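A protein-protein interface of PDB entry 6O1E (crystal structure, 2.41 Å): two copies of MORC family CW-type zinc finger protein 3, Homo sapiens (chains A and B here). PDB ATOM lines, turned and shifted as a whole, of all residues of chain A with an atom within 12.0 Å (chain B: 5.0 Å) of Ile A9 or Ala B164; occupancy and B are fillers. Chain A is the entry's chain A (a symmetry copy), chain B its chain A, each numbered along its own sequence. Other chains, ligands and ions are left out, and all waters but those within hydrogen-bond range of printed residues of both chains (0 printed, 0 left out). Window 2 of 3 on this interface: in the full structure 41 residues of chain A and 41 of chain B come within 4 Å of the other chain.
The side-chain carboxylate of Glu B161 lies within hydrogen-bond range of the backbone NH of Ile A9, 2.5 Å away.
The backbone NH (N) of Val B145 lies within hydrogen-bond range of the backbone carbonyl oxygen (O) of Arg A10 (2.9 Å).
OE2 of Glu B161 sits at hydrogen-bond distance from N of Arg A10 (3.4 Å).
The backbone carbonyl oxygen of Glu B161 is in hydrogen-bond range of the side-chain hydroxyl of Ser B165, at 2.8 Å.
Tyr B134 touches Ile A9 (OH to CD1, 3.9 Å).
C of Val B145 touches CG2 of Ile A9, at 3.9 Å.
Ile A9 touches Pro B146.
O of Ala B164 touches CD1 of Ile A9, 3.3 Å away.
Ser B165 touches Ile A9.
Arg A10 touches Val B144 (O to CA, 3.4 Å).
Val B144 touches Leu A11 (CG1 to CD2, 3.5 Å).
Val B145 touches Ser A12.
Ile A9 touches just these residues of chain B: Tyr B134 (3.9 Å), Val B145 (3.9 Å), Pro B146 (3.6 Å), Glu B161 (2.5 Å), Ala B164 (3.3 Å) and Ser B165 (3.7 Å).
Printed residues of chain B within 4 Å of Arg A10: Val B144 (3.4 Å), Val B145 (2.9 Å) and Glu B161 (3.4 Å).
Of the printed residues of chain B, Leu A11 touches Val B144 (3.5 Å).
Printed residues of chain B within 4 Å of Ser A12: Val B145.
Printed residues of chain A within 4 Å of Tyr B134: Ile A9 (3.9 Å).
Val B144 touches just these residues of chain A: Arg A10 and Leu A11.
Of chain A, only Ile A9 (2.5 Å) and Arg A10 (3.4 Å) come within 4 Å of Glu B161.
No residue of chain A comes within 4 Å of Ser B162.
No residue of chain A comes within 4 Å of Lys B163.
Ala B164 touches just one residue of chain A: Ile A9.
Of the printed residues of chain A, Ser B165 touches Ile A9 (3.7 Å).
No residue of chain A comes within 4 Å of Leu B166.
Ala B168 touches none of the printed residues of chain A.
The nearest printed residue of chain B that does not touch Ile A9 is Ala B168 (4.1 Å).
Printed residues of chain A that touch a printed residue of chain B: Ile A9, Arg A10, Leu A11 and Ser A12.
Printed residues of chain B that touch a printed residue of chain A: Tyr B134, Val B144, Val B145, Pro B146, Glu B161, Ala B164 and Ser B165.
Along chain B the printed residues that touch a printed residue of chain A span positions 134 to 165.
Among the printed residues, 11 pairs touch across the chains.
No position is printed for both chains.
Of the 11 pairs that touch across the chains among the printed residues, none has its exchanged pair printed and touching as well.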
ATOM      1  N   ILE A   9      -3.702   1.243   5.175  1.00  0.00           N
ATOM      2  CA  ILE A   9      -4.832   0.308   5.198  1.00  0.00           C
ATOM      3  C   ILE A   9      -6.061   0.913   4.521  1.00  0.00           C
ATOM      4  O   ILE A   9      -6.482   2.019   4.860  1.00  0.00           O
ATOM      5  CB  ILE A   9      -5.148  -0.134   6.622  1.00  0.00           C
ATOM      6  CG1 ILE A   9      -3.892  -0.729   7.261  1.00  0.00           C
ATOM      7  CG2 ILE A   9      -6.321  -1.122   6.621  1.00  0.00           C
ATOM      8  CD1 ILE A   9      -4.057  -1.120   8.704  1.00  0.00           C
ATOM      9  N   ARG A  10      -6.647   0.176   3.575  1.00  0.00           N
ATOM     10  CA  ARG A  10      -7.631   0.767   2.676  1.00  0.00           C
ATOM     11  C   ARG A  10      -9.024   0.834   3.304  1.00  0.00           C
ATOM     12  O   ARG A  10      -9.442  -0.064   4.043  1.00  0.00           O
ATOM     13  CB  ARG A  10      -7.673  -0.005   1.355  1.00  0.00           C
ATOM     14  CG  ARG A  10      -6.935   0.712   0.226  1.00  0.00           C
ATOM     15  CD  ARG A  10      -7.627   0.528  -1.109  1.00  0.00           C
ATOM     16  NE  ARG A  10      -7.238  -0.735  -1.729  1.00  0.00           N
ATOM     17  CZ  ARG A  10      -7.739  -1.198  -2.874  1.00  0.00           C
ATOM     18  NH1 ARG A  10      -7.319  -2.369  -3.349  1.00  0.00           N
ATOM     19  NH2 ARG A  10      -8.664  -0.508  -3.543  1.00  0.00           N
ATOM     20  N   LEU A  11      -9.729   1.929   3.017  1.00  0.00           N
ATOM     21  CA  LEU A  11     -11.115   2.077   3.443  1.00  0.00           C
ATOM     22  C   LEU A  11     -12.002   1.086   2.700  1.00  0.00           C
ATOM     23  O   LEU A  11     -11.815   0.837   1.505  1.00  0.00           O
ATOM     24  CB  LEU A  11     -11.621   3.492   3.161  1.00  0.00           C
ATOM     25  CG  LEU A  11     -11.133   4.735   3.897  1.00  0.00           C
ATOM     26  CD1 LEU A  11     -11.972   5.944   3.484  1.00  0.00           C
ATOM     27  CD2 LEU A  11     -11.217   4.541   5.395  1.00  0.00           C
ATOM     28  N   SER A  12     -12.987   0.532   3.404  1.00  0.00           N
ATOM     29  CA  SER A  12     -14.039  -0.216   2.724  1.00  0.00           C
ATOM     30  C   SER A  12     -14.807   0.724   1.805  1.00  0.00           C
ATOM     31  O   SER A  12     -15.200   1.822   2.215  1.00  0.00           O
ATOM     32  CB  SER A  12     -14.980  -0.856   3.740  1.00  0.00           C
ATOM     33  OG  SER A  12     -15.827  -1.793   3.105  1.00  0.00           O
ATOM     34  N   ALA A  13     -14.986   0.315   0.551  1.00  0.00           N
ATOM     35  CA  ALA A  13     -15.588   1.195  -0.442  1.00  0.00           C
ATOM     36  C   ALA A  13     -17.104   1.017  -0.488  1.00  0.00           C
ATOM     37  O   ALA A  13     -17.661   0.004  -0.047  1.00  0.00           O
ATOM     38  CB  ALA A  13     -15.000   0.938  -1.832  1.00  0.00           C
ATOM     39  N   HIS A 142     -17.590   5.228  -6.699  1.00  0.00           N
ATOM     40  CA  HIS A 142     -17.866   5.483  -5.295  1.00  0.00           C
ATOM     41  C   HIS A 142     -19.072   6.407  -5.191  1.00  0.00           C
ATOM     42  O   HIS A 142     -19.397   7.145  -6.129  1.00  0.00           O
ATOM     43  CB  HIS A 142     -16.665   6.104  -4.578  1.00  0.00           C
ATOM     44  CG  HIS A 142     -15.438   5.249  -4.615  1.00  0.00           C
ATOM     45  ND1 HIS A 142     -15.280   4.139  -3.813  1.00  0.00           N
ATOM     46  CD2 HIS A 142     -14.306   5.345  -5.351  1.00  0.00           C
ATOM     47  CE1 HIS A 142     -14.107   3.582  -4.061  1.00  0.00           C
ATOM     48  NE2 HIS A 142     -13.494   4.298  -4.986  1.00  0.00           N
ATOM     49  N   TYR B 134     -12.075  -5.094  16.073  1.00  0.00           N
ATOM     50  CA  TYR B 134     -10.900  -4.340  15.642  1.00  0.00           C
ATOM     51  C   TYR B 134     -11.236  -2.870  15.437  1.00  0.00           C
ATOM     52  O   TYR B 134     -10.542  -1.986  15.947  1.00  0.00           O
ATOM     53  CB  TYR B 134     -10.332  -4.964  14.366  1.00  0.00           C
ATOM     54  CG  TYR B 134      -9.383  -4.087  13.581  1.00  0.00           C
ATOM     55  CD1 TYR B 134      -9.679  -3.712  12.275  1.00  0.00           C
ATOM     56  CD2 TYR B 134      -8.186  -3.643  14.137  1.00  0.00           C
ATOM     57  CE1 TYR B 134      -8.816  -2.922  11.540  1.00  0.00           C
ATOM     58  CE2 TYR B 134      -7.310  -2.848  13.413  1.00  0.00           C
ATOM     59  CZ  TYR B 134      -7.630  -2.487  12.111  1.00  0.00           C
ATOM     60  OH  TYR B 134      -6.779  -1.689  11.374  1.00  0.00           O
ATOM     61  N   VAL B 144     -12.331   0.096   7.756  1.00  0.00           N
ATOM     62  CA  VAL B 144     -11.090  -0.154   7.036  1.00  0.00           C
ATOM     63  C   VAL B 144     -10.883  -1.656   6.983  1.00  0.00           C
ATOM     64  O   VAL B 144     -11.269  -2.391   7.899  1.00  0.00           O
ATOM     65  CB  VAL B 144      -9.877   0.547   7.693  1.00  0.00           C
ATOM     66  CG1 VAL B 144     -10.025   2.048   7.570  1.00  0.00           C
ATOM     67  CG2 VAL B 144      -9.743   0.136   9.168  1.00  0.00           C
ATOM     68  N   VAL B 145     -10.265  -2.116   5.906  1.00  0.00           N
ATOM     69  CA  VAL B 145     -10.197  -3.552   5.688  1.00  0.00           C
ATOM     70  C   VAL B 145      -8.747  -3.950   5.442  1.00  0.00           C
ATOM     71  O   VAL B 145      -8.265  -3.891   4.301  1.00  0.00           O
ATOM     72  CB  VAL B 145     -11.131  -3.971   4.539  1.00  0.00           C
ATOM     73  CG1 VAL B 145     -12.553  -4.102   5.057  1.00  0.00           C
ATOM     74  CG2 VAL B 145     -11.086  -2.947   3.408  1.00  0.00           C
ATOM     75  N   PRO B 146      -8.016  -4.343   6.482  1.00  0.00           N
ATOM     76  CA  PRO B 146      -6.636  -4.815   6.284  1.00  0.00           C
ATOM     77  C   PRO B 146      -6.590  -5.988   5.318  1.00  0.00           C
ATOM     78  O   PRO B 146      -7.192  -7.041   5.560  1.00  0.00           O
ATOM     79  CB  PRO B 146      -6.199  -5.232   7.694  1.00  0.00           C
ATOM     80  CG  PRO B 146      -7.061  -4.410   8.616  1.00  0.00           C
ATOM     81  CD  PRO B 146      -8.373  -4.208   7.907  1.00  0.00           C
ATOM     82  N   ALA B 160       3.434  -1.787   0.358  1.00  0.00           N
ATOM     83  CA  ALA B 160       2.935  -0.484   0.792  1.00  0.00           C
ATOM     84  C   ALA B 160       1.780  -0.635   1.771  1.00  0.00           C
ATOM     85  O   ALA B 160       1.926  -0.343   2.961  1.00  0.00           O
ATOM     86  CB  ALA B 160       2.499   0.348  -0.419  1.00  0.00           C
ATOM     87  N   GLU B 161       0.638  -1.122   1.300  1.00  0.00           N
ATOM     88  CA  GLU B 161      -0.484  -1.322   2.205  1.00  0.00           C
ATOM     89  C   GLU B 161      -0.442  -2.668   2.927  1.00  0.00           C
ATOM     90  O   GLU B 161      -1.281  -2.900   3.804  1.00  0.00           O
ATOM     91  CB  GLU B 161      -1.809  -1.163   1.449  1.00  0.00           C
ATOM     92  CG  GLU B 161      -2.064   0.275   0.997  1.00  0.00           C
ATOM     93  CD  GLU B 161      -2.382   1.217   2.158  1.00  0.00           C
ATOM     94  OE1 GLU B 161      -1.491   1.995   2.580  1.00  0.00           O
ATOM     95  OE2 GLU B 161      -3.530   1.188   2.638  1.00  0.00           O
ATOM     96  N   SER B 162       0.516  -3.546   2.612  1.00  0.00           N
ATOM     97  CA  SER B 162       0.598  -4.831   3.300  1.00  0.00           C
ATOM     98  C   SER B 162       1.279  -4.749   4.662  1.00  0.00           C
ATOM     99  O   SER B 162       1.101  -5.667   5.474  1.00  0.00           O
ATOM    100  CB  SER B 162       1.344  -5.854   2.444  1.00  0.00           C
ATOM    101  OG  SER B 162       0.491  -6.433   1.476  1.00  0.00           O
ATOM    102  N   LYS B 163       2.066  -3.698   4.924  1.00  0.00           N
ATOM    103  CA  LYS B 163       2.779  -3.579   6.194  1.00  0.00           C
ATOM    104  C   LYS B 163       1.812  -3.256   7.324  1.00  0.00           C
ATOM    105  O   LYS B 163       1.700  -4.019   8.293  1.00  0.00           O
ATOM    106  CB  LYS B 163       3.870  -2.502   6.134  1.00  0.00           C
ATOM    107  CG  LYS B 163       3.442  -1.185   5.484  1.00  0.00           C
ATOM    108  CD  LYS B 163       4.148   0.017   6.120  1.00  0.00           C
ATOM    109  CE  LYS B 163       5.674  -0.028   5.977  1.00  0.00           C
ATOM    110  NZ  LYS B 163       6.286   1.349   6.000  1.00  0.00           N
ATOM    111  N   ALA B 164       1.120  -2.118   7.208  1.00  0.00           N
ATOM    112  CA  ALA B 164       0.148  -1.749   8.226  1.00  0.00           C
ATOM    113  C   ALA B 164      -0.960  -2.787   8.329  1.00  0.00           C
ATOM    114  O   ALA B 164      -1.475  -3.037   9.429  1.00  0.00           O
ATOM    115  CB  ALA B 164      -0.425  -0.367   7.927  1.00  0.00           C
ATOM    116  N   SER B 165      -1.317  -3.420   7.206  1.00  0.00           N
ATOM    117  CA  SER B 165      -2.366  -4.434   7.227  1.00  0.00           C
ATOM    118  C   SER B 165      -1.935  -5.629   8.054  1.00  0.00           C
ATOM    119  O   SER B 165      -2.694  -6.118   8.898  1.00  0.00           O
ATOM    120  CB  SER B 165      -2.723  -4.878   5.807  1.00  0.00           C
ATOM    121  OG  SER B 165      -3.495  -3.899   5.124  1.00  0.00           O
ATOM    122  N   LEU B 166      -0.710  -6.104   7.828  1.00  0.00           N
ATOM    123  CA  LEU B 166      -0.203  -7.250   8.576  1.00  0.00           C
ATOM    124  C   LEU B 166      -0.051  -6.923  10.059  1.00  0.00           C
ATOM    125  O   LEU B 166      -0.310  -7.773  10.921  1.00  0.00           O
ATOM    126  CB  LEU B 166       1.123  -7.700   7.980  1.00  0.00           C
ATOM    127  CG  LEU B 166       1.423  -9.193   8.085  1.00  0.00           C
ATOM    128  CD1 LEU B 166       2.634  -9.459   7.257  1.00  0.00           C
ATOM    129  CD2 LEU B 166       1.673  -9.638   9.508  1.00  0.00           C
ATOM    130  N   ALA B 167       0.368  -5.699  10.378  1.00  0.00           N
ATOM    131  CA  ALA B 167       0.434  -5.295  11.780  1.00  0.00           C
ATOM    132  C   ALA B 167      -0.939  -5.393  12.442  1.00  0.00           C
ATOM    133  O   ALA B 167      -1.082  -5.972  13.529  1.00  0.00           O
ATOM    134  CB  ALA B 167       0.991  -3.875  11.896  1.00  0.00           C
ATOM    135  N   ALA B 168      -1.965  -4.839  11.787  1.00  0.00           N
ATOM    136  CA  ALA B 168      -3.318  -4.911  12.332  1.00  0.00           C
ATOM    137  C   ALA B 168      -3.790  -6.354  12.454  1.00  0.00           C
ATOM    138  O   ALA B 168      -4.374  -6.742  13.474  1.00  0.00           O
ATOM    139  CB  ALA B 168      -4.276  -4.097  11.458  1.00  0.00           C
